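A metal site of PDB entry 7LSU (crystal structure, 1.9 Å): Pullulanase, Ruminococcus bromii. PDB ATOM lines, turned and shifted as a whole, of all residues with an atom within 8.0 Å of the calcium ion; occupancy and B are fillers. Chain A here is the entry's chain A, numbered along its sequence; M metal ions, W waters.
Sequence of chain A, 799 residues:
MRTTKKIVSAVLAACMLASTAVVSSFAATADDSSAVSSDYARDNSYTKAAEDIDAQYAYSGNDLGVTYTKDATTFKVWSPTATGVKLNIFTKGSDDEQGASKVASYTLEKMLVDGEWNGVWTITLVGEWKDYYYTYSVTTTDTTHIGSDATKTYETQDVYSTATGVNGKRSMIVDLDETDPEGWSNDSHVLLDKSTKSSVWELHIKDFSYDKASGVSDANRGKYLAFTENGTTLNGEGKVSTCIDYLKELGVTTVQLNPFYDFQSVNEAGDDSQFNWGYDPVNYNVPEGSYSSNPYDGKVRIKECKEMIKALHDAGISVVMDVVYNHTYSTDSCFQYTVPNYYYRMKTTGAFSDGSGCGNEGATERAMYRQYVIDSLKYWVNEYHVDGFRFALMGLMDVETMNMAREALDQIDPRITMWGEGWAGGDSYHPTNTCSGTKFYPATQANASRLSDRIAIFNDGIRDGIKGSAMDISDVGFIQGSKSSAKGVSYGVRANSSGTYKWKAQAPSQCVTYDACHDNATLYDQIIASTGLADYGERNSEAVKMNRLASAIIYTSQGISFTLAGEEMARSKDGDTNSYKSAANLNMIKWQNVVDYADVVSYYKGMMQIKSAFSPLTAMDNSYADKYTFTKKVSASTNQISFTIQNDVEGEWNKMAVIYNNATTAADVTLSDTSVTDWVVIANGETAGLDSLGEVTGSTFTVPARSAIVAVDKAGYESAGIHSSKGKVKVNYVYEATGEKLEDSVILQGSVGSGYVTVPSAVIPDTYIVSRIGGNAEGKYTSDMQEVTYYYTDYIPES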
ATOM      1  N   THR A 164      -3.131  -2.526 -25.254  1.00  0.00           N
ATOM      2  CA  THR A 164      -2.067  -3.495 -25.497  1.00  0.00           C
ATOM      3  C   THR A 164      -2.666  -4.900 -25.622  1.00  0.00           C
ATOM      4  O   THR A 164      -3.835  -5.123 -25.295  1.00  0.00           O
ATOM      5  CB  THR A 164      -1.015  -3.496 -24.385  1.00  0.00           C
ATOM      6  OG1 THR A 164      -1.652  -3.909 -23.173  1.00  0.00           O
ATOM      7  CG2 THR A 164      -0.348  -2.153 -24.191  1.00  0.00           C
ATOM      8  N   GLY A 165      -1.834  -5.834 -26.103  1.00  0.00           N
ATOM      9  CA  GLY A 165      -2.115  -7.258 -26.040  1.00  0.00           C
ATOM     10  C   GLY A 165      -1.823  -7.801 -24.652  1.00  0.00           C
ATOM     11  O   GLY A 165      -1.796  -7.060 -23.677  1.00  0.00           O
ATOM     12  N   VAL A 166      -1.592  -9.116 -24.579  1.00  0.00           N
ATOM     13  CA  VAL A 166      -1.349  -9.808 -23.312  1.00  0.00           C
ATOM     14  C   VAL A 166       0.025  -9.382 -22.766  1.00  0.00           C
ATOM     15  O   VAL A 166       1.016  -9.360 -23.498  1.00  0.00           O
ATOM     16  CB  VAL A 166      -1.482 -11.337 -23.462  1.00  0.00           C
ATOM     17  CG1 VAL A 166      -0.422 -11.924 -24.393  1.00  0.00           C
ATOM     18  CG2 VAL A 166      -1.454 -12.034 -22.109  1.00  0.00           C
ATOM     19  N   ASN A 167       0.039  -9.010 -21.478  1.00  0.00           N
ATOM     20  CA  ASN A 167       1.238  -8.687 -20.683  1.00  0.00           C
ATOM     21  C   ASN A 167       1.895  -7.387 -21.180  1.00  0.00           C
ATOM     22  O   ASN A 167       3.060  -7.132 -20.867  1.00  0.00           O
ATOM     23  CB  ASN A 167       2.214  -9.863 -20.635  1.00  0.00           C
ATOM     24  CG  ASN A 167       1.758 -10.980 -19.720  1.00  0.00           C
ATOM     25  OD1 ASN A 167       1.028 -10.747 -18.758  1.00  0.00           O
ATOM     26  ND2 ASN A 167       2.184 -12.200 -20.010  1.00  0.00           N
ATOM     27  N   GLY A 168       1.142  -6.561 -21.923  1.00  0.00           N
ATOM     28  CA  GLY A 168       1.483  -5.164 -22.211  1.00  0.00           C
ATOM     29  C   GLY A 168       2.787  -4.982 -22.985  1.00  0.00           C
ATOM     30  O   GLY A 168       3.482  -3.981 -22.779  1.00  0.00           O
ATOM     31  N   TYR A 261      -4.816   0.270 -13.693  1.00  0.00           N
ATOM     32  CA  TYR A 261      -3.873   0.469 -14.800  1.00  0.00           C
ATOM     33  C   TYR A 261      -3.087  -0.836 -14.983  1.00  0.00           C
ATOM     34  O   TYR A 261      -3.091  -1.687 -14.106  1.00  0.00           O
ATOM     35  CB  TYR A 261      -2.924   1.637 -14.521  1.00  0.00           C
ATOM     36  CG  TYR A 261      -2.075   1.444 -13.293  1.00  0.00           C
ATOM     37  CD1 TYR A 261      -0.909   0.709 -13.347  1.00  0.00           C
ATOM     38  CD2 TYR A 261      -2.461   1.978 -12.067  1.00  0.00           C
ATOM     39  CE1 TYR A 261      -0.134   0.497 -12.210  1.00  0.00           C
ATOM     40  CE2 TYR A 261      -1.689   1.783 -10.923  1.00  0.00           C
ATOM     41  CZ  TYR A 261      -0.525   1.045 -11.001  1.00  0.00           C
ATOM     42  OH  TYR A 261       0.241   0.839  -9.892  1.00  0.00           O
ATOM     43  N   ASP A 262      -2.412  -0.978 -16.126  1.00  0.00           N
ATOM     44  CA  ASP A 262      -1.699  -2.215 -16.461  1.00  0.00           C
ATOM     45  C   ASP A 262      -0.415  -2.322 -15.644  1.00  0.00           C
ATOM     46  O   ASP A 262       0.481  -1.476 -15.762  1.00  0.00           O
ATOM     47  CB  ASP A 262      -1.403  -2.288 -17.969  1.00  0.00           C
ATOM     48  CG  ASP A 262      -0.848  -3.632 -18.408  1.00  0.00           C
ATOM     49  OD1 ASP A 262      -1.261  -4.656 -17.842  1.00  0.00           O
ATOM     50  OD2 ASP A 262       0.013  -3.636 -19.325  1.00  0.00           O
ATOM     51  N   PHE A 263      -0.323  -3.366 -14.806  1.00  0.00           N
ATOM     52  CA  PHE A 263       0.855  -3.642 -13.976  1.00  0.00           C
ATOM     53  C   PHE A 263       1.505  -4.958 -14.407  1.00  0.00           C
ATOM     54  O   PHE A 263       0.937  -5.705 -15.211  1.00  0.00           O
ATOM     55  CB  PHE A 263       0.484  -3.602 -12.488  1.00  0.00           C
ATOM     56  CG  PHE A 263      -0.665  -4.496 -12.068  1.00  0.00           C
ATOM     57  CD1 PHE A 263      -0.464  -5.844 -11.822  1.00  0.00           C
ATOM     58  CD2 PHE A 263      -1.937  -3.974 -11.891  1.00  0.00           C
ATOM     59  CE1 PHE A 263      -1.511  -6.662 -11.411  1.00  0.00           C
ATOM     60  CE2 PHE A 263      -2.984  -4.792 -11.479  1.00  0.00           C
ATOM     61  CZ  PHE A 263      -2.772  -6.131 -11.252  1.00  0.00           C
ATOM     62  N   GLN A 264       2.698  -5.231 -13.865  1.00  0.00           N
ATOM     63  CA  GLN A 264       3.602  -6.279 -14.355  1.00  0.00           C
ATOM     64  C   GLN A 264       3.348  -7.625 -13.657  1.00  0.00           C
ATOM     65  O   GLN A 264       3.494  -8.682 -14.280  1.00  0.00           O
ATOM     66  CB  GLN A 264       5.059  -5.851 -14.132  1.00  0.00           C
ATOM     67  CG  GLN A 264       6.086  -6.826 -14.688  1.00  0.00           C
ATOM     68  CD  GLN A 264       6.478  -7.913 -13.713  1.00  0.00           C
ATOM     69  OE1 GLN A 264       6.238  -7.831 -12.509  1.00  0.00           O
ATOM     70  NE2 GLN A 264       7.106  -8.954 -14.242  1.00  0.00           N
ATOM     71  N   SER A 265       2.991  -7.565 -12.372  1.00  0.00           N
ATOM     72  CA  SER A 265       3.273  -8.634 -11.399  1.00  0.00           C
ATOM     73  C   SER A 265       2.231  -9.765 -11.414  1.00  0.00           C
ATOM     74  O   SER A 265       2.313 -10.670 -10.574  1.00  0.00           O
ATOM     75  CB  SER A 265       3.405  -8.041 -10.014  1.00  0.00           C
ATOM     76  OG  SER A 265       2.309  -7.177  -9.733  1.00  0.00           O
ATOM     77  N   VAL A 266       1.272  -9.739 -12.348  1.00  0.00           N
ATOM     78  CA  VAL A 266       0.390 -10.880 -12.609  1.00  0.00           C
ATOM     79  C   VAL A 266       0.558 -11.302 -14.069  1.00  0.00           C
ATOM     80  O   VAL A 266       0.374 -10.488 -14.978  1.00  0.00           O
ATOM     81  CB  VAL A 266      -1.086 -10.547 -12.283  1.00  0.00           C
ATOM     82  CG1 VAL A 266      -2.050 -11.528 -12.935  1.00  0.00           C
ATOM     83  CG2 VAL A 266      -1.332 -10.483 -10.782  1.00  0.00           C
ATOM     84  N   ASN A 267       0.932 -12.570 -14.286  1.00  0.00           N
ATOM     85  CA  ASN A 267       1.030 -13.133 -15.629  1.00  0.00           C
ATOM     86  C   ASN A 267      -0.385 -13.370 -16.163  1.00  0.00           C
ATOM     87  O   ASN A 267      -1.107 -14.235 -15.680  1.00  0.00           O
ATOM     88  CB  ASN A 267       1.864 -14.415 -15.655  1.00  0.00           C
ATOM     89  CG  ASN A 267       2.024 -15.001 -17.042  1.00  0.00           C
ATOM     90  OD1 ASN A 267       1.850 -14.292 -18.039  1.00  0.00           O
ATOM     91  ND2 ASN A 267       2.360 -16.278 -17.128  1.00  0.00           N
ATOM     92  N   GLU A 268      -0.745 -12.589 -17.188  1.00  0.00           N
ATOM     93  CA  GLU A 268      -2.113 -12.531 -17.720  1.00  0.00           C
ATOM     94  C   GLU A 268      -2.444 -13.806 -18.507  1.00  0.00           C
ATOM     95  O   GLU A 268      -3.611 -14.078 -18.773  1.00  0.00           O
ATOM     96  CB  GLU A 268      -2.289 -11.281 -18.583  1.00  0.00           C
ATOM     97  CG  GLU A 268      -2.138  -9.983 -17.800  1.00  0.00           C
ATOM     98  CD  GLU A 268      -2.173  -8.718 -18.639  1.00  0.00           C
ATOM     99  OE1 GLU A 268      -2.303  -8.828 -19.878  1.00  0.00           O
ATOM    100  OE2 GLU A 268      -2.072  -7.620 -18.048  1.00  0.00           O
ATOM    101  N   ASP A 280       3.060  -1.842  -9.624  1.00  0.00           N
ATOM    102  CA  ASP A 280       4.163  -2.258 -10.510  1.00  0.00           C
ATOM    103  C   ASP A 280       3.829  -1.827 -11.932  1.00  0.00           C
ATOM    104  O   ASP A 280       3.627  -2.657 -12.808  1.00  0.00           O
ATOM    105  CB  ASP A 280       4.363  -3.777 -10.436  1.00  0.00           C
ATOM    106  CG  ASP A 280       4.581  -4.320  -9.029  1.00  0.00           C
ATOM    107  OD1 ASP A 280       5.528  -3.854  -8.366  1.00  0.00           O
ATOM    108  OD2 ASP A 280       3.796  -5.196  -8.610  1.00  0.00           O
ATOM    109  N   PRO A 281       3.771  -0.500 -12.227  1.00  0.00           N
ATOM    110  CA  PRO A 281       3.226  -0.010 -13.495  1.00  0.00           C
ATOM    111  C   PRO A 281       4.040  -0.352 -14.745  1.00  0.00           C
ATOM    112  O   PRO A 281       5.276  -0.305 -14.720  1.00  0.00           O
ATOM    113  CB  PRO A 281       3.197   1.521 -13.313  1.00  0.00           C
ATOM    114  CG  PRO A 281       3.308   1.726 -11.818  1.00  0.00           C
ATOM    115  CD  PRO A 281       4.194   0.596 -11.347  1.00  0.00           C
ATOM    116  N   VAL A 282       3.336  -0.695 -15.831  1.00  0.00           N
ATOM    117  CA  VAL A 282       3.916  -0.969 -17.157  1.00  0.00           C
ATOM    118  C   VAL A 282       3.303  -0.017 -18.183  1.00  0.00           C
ATOM    119  O   VAL A 282       4.024   0.625 -18.942  1.00  0.00           O
ATOM    120  CB  VAL A 282       3.730  -2.445 -17.560  1.00  0.00           C
ATOM    121  CG1 VAL A 282       4.404  -2.744 -18.901  1.00  0.00           C
ATOM    122  CG2 VAL A 282       4.245  -3.406 -16.501  1.00  0.00           C
ATOM    123  N   ASN A 283       1.963   0.038 -18.235  1.00  0.00           N
ATOM    124  CA  ASN A 283       1.220   0.903 -19.140  1.00  0.00           C
ATOM    125  C   ASN A 283       0.190   1.716 -18.339  1.00  0.00           C
ATOM    126  O   ASN A 283      -0.791   1.170 -17.844  1.00  0.00           O
ATOM    127  CB  ASN A 283       0.542   0.112 -20.263  1.00  0.00           C
ATOM    128  CG  ASN A 283       1.544  -0.599 -21.156  1.00  0.00           C
ATOM    129  OD1 ASN A 283       2.326   0.039 -21.849  1.00  0.00           O
ATOM    130  ND2 ASN A 283       1.522  -1.927 -21.140  1.00  0.00           N
ATOM    131  N   VAL A 286      -3.560   2.119 -19.948  1.00  0.00           N
ATOM    132  CA  VAL A 286      -4.157   0.865 -20.408  1.00  0.00           C
ATOM    133  C   VAL A 286      -4.669   0.093 -19.189  1.00  0.00           C
ATOM    134  O   VAL A 286      -3.939  -0.048 -18.213  1.00  0.00           O
ATOM    135  CB  VAL A 286      -3.144   0.025 -21.213  1.00  0.00           C
ATOM    136  CG1 VAL A 286      -3.711  -1.341 -21.602  1.00  0.00           C
ATOM    137  CG2 VAL A 286      -2.664   0.764 -22.453  1.00  0.00           C
ATOM    138  N   PRO A 287      -5.936  -0.393 -19.191  1.00  0.00           N
ATOM    139  CA  PRO A 287      -6.439  -1.223 -18.093  1.00  0.00           C
ATOM    140  C   PRO A 287      -5.617  -2.498 -17.866  1.00  0.00           C
ATOM    141  O   PRO A 287      -4.987  -3.012 -18.790  1.00  0.00           O
ATOM    142  CB  PRO A 287      -7.860  -1.586 -18.538  1.00  0.00           C
ATOM    143  CG  PRO A 287      -8.248  -0.501 -19.522  1.00  0.00           C
ATOM    144  CD  PRO A 287      -6.957  -0.128 -20.214  1.00  0.00           C
ATOM    145  N   GLU A 288      -5.646  -3.002 -16.624  1.00  0.00           N
ATOM    146  CA  GLU A 288      -5.000  -4.269 -16.260  1.00  0.00           C
ATOM    147  C   GLU A 288      -5.728  -5.411 -16.966  1.00  0.00           C
ATOM    148  O   GLU A 288      -6.954  -5.442 -17.024  1.00  0.00           O
ATOM    149  CB  GLU A 288      -5.006  -4.437 -14.730  1.00  0.00           C
ATOM    150  CG  GLU A 288      -4.657  -5.845 -14.261  1.00  0.00           C
ATOM    151  CD  GLU A 288      -3.290  -6.370 -14.663  1.00  0.00           C
ATOM    152  OE1 GLU A 288      -2.420  -5.553 -15.028  1.00  0.00           O
ATOM    153  OE2 GLU A 288      -3.098  -7.600 -14.604  1.00  0.00           O
ATOM    154  N   GLY A 289      -4.943  -6.359 -17.514  1.00  0.00           N
ATOM    155  CA  GLY A 289      -5.458  -7.448 -18.338  1.00  0.00           C
ATOM    156  C   GLY A 289      -6.089  -8.569 -17.533  1.00  0.00           C
ATOM    157  O   GLY A 289      -7.082  -9.155 -17.969  1.00  0.00           O
ATOM    158  N   SER A 290      -5.540  -8.853 -16.349  1.00  0.00           N
ATOM    159  CA  SER A 290      -5.908 -10.025 -15.549  1.00  0.00           C
ATOM    160  C   SER A 290      -7.324  -9.898 -14.971  1.00  0.00           C
ATOM    161  O   SER A 290      -7.930 -10.912 -14.617  1.00  0.00           O
ATOM    162  CB  SER A 290      -4.898 -10.273 -14.456  1.00  0.00           C
ATOM    163  OG  SER A 290      -4.887  -9.215 -13.505  1.00  0.00           O
ATOM    164  N   TYR A 291      -7.851  -8.674 -14.869  1.00  0.00           N
ATOM    165  CA  TYR A 291      -9.203  -8.426 -14.338  1.00  0.00           C
ATOM    166  C   TYR A 291     -10.253  -8.541 -15.450  1.00  0.00           C
ATOM    167  O   TYR A 291     -11.451  -8.503 -15.165  1.00  0.00           O
ATOM    168  CB  TYR A 291      -9.278  -7.064 -13.648  1.00  0.00           C
ATOM    169  CG  TYR A 291      -8.354  -6.907 -12.472  1.00  0.00           C
ATOM    170  CD1 TYR A 291      -8.197  -7.923 -11.538  1.00  0.00           C
ATOM    171  CD2 TYR A 291      -7.636  -5.738 -12.275  1.00  0.00           C
ATOM    172  CE1 TYR A 291      -7.338  -7.794 -10.458  1.00  0.00           C
ATOM    173  CE2 TYR A 291      -6.780  -5.588 -11.200  1.00  0.00           C
ATOM    174  CZ  TYR A 291      -6.633  -6.618 -10.281  1.00  0.00           C
ATOM    175  OH  TYR A 291      -5.787  -6.481  -9.220  1.00  0.00           O
ATOM    176  N   PRO A 295      -7.394 -11.105 -22.028  1.00  0.00           N
ATOM    177  CA  PRO A 295      -6.313 -10.130 -22.134  1.00  0.00           C
ATOM    178  C   PRO A 295      -5.582 -10.103 -23.498  1.00  0.00           C
ATOM    179  O   PRO A 295      -4.752  -9.214 -23.725  1.00  0.00           O
ATOM    180  CB  PRO A 295      -5.347 -10.572 -21.027  1.00  0.00           C
ATOM    181  CG  PRO A 295      -5.519 -12.079 -20.961  1.00  0.00           C
ATOM    182  CD  PRO A 295      -6.942 -12.362 -21.400  1.00  0.00           C
ATOM    183  N   ARG A 301     -10.748  -5.746 -22.431  1.00  0.00           N
ATOM    184  CA  ARG A 301     -10.459  -5.227 -21.088  1.00  0.00           C
ATOM    185  C   ARG A 301     -10.922  -3.766 -20.965  1.00  0.00           C
ATOM    186  O   ARG A 301     -11.292  -3.336 -19.882  1.00  0.00           O
ATOM    187  CB  ARG A 301      -8.959  -5.357 -20.760  1.00  0.00           C
ATOM    188  CG  ARG A 301      -8.041  -4.427 -21.542  1.00  0.00           C
ATOM    189  CD  ARG A 301      -6.609  -4.533 -21.081  1.00  0.00           C
ATOM    190  NE  ARG A 301      -5.926  -5.711 -21.591  1.00  0.00           N
ATOM    191  CZ  ARG A 301      -4.650  -6.017 -21.364  1.00  0.00           C
ATOM    192  NH1 ARG A 301      -3.919  -5.223 -20.601  1.00  0.00           N
ATOM    193  NH2 ARG A 301      -4.117  -7.093 -21.889  1.00  0.00           N
HETATM  194 CA    CA M   1      -0.536  -6.586 -16.673  1.00  0.00          CA
HETATM  195  O   HOH W   1       1.018  -8.657 -17.014  1.00  0.00           O
HETATM  196  O   HOH W   2      -0.543  -8.107 -14.851  1.00  0.00           O
HETATM  197  O   HOH W   3       1.268  -6.008 -18.418  1.00  0.00           O
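ND2 of Asn 283 is in hydrogen-bond range of OD2 of Asp 262 (2.9 Å). OG of Ser 290 lies within hydrogen-bond range of OE2 of Glu 288 (2.6 Å). The backbone NH (N) of Asp 262 sits at hydrogen-bond distance from the backbone carbonyl oxygen (O) of Val 286 (2.7 Å). OD1 of Asp 262 lies close to NH1 of Arg 301, at 3.9 Å. The backbone NH (N) of Val 282 is in hydrogen-bond range of the backbone carbonyl oxygen (O) of Asp 262 (3.0 Å). OE1 of Glu 268 lies within salt-bridge range of NH2 of Arg 301 (3.2 Å). The backbone NH (N) of Asn 167 sits at hydrogen-bond distance from the side-chain carboxylate (OE1) of Glu 268 (2.8 Å). OE2 of Glu 268 sits close to N of Gly 289, at 3.2 Å.
Of the 25 residues printed, 4 come within 4 Å of the calcium ion. The nearest printed residue that does not touch the calcium ion is Val 266 (4.4 Å).
The calcium ion is bound by O of Phe 263 (2.3 Å), OE2 of Glu 268 (2.3 Å), OD1 of Asp 262 (2.4 Å), water W2 (2.4 Å), water W3 (2.6 Å), water W1 (2.6 Å) and OE1 of Glu 288 (2.7 Å). The calcium ion has seven donor atoms within binding distance.
Water W2 lies within hydrogen-bond range of O of Val 266 and OE2 of Glu 288. Water W1 lies within hydrogen-bond range of OD1 of Asn 167 (2.7 Å) and O of Val 266 (2.8 Å). Water W3 bridges the side-chain carboxylate of Asp 262 (2.8 Å) and the backbone carbonyl oxygen of Asn 167 (3.2 Å).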
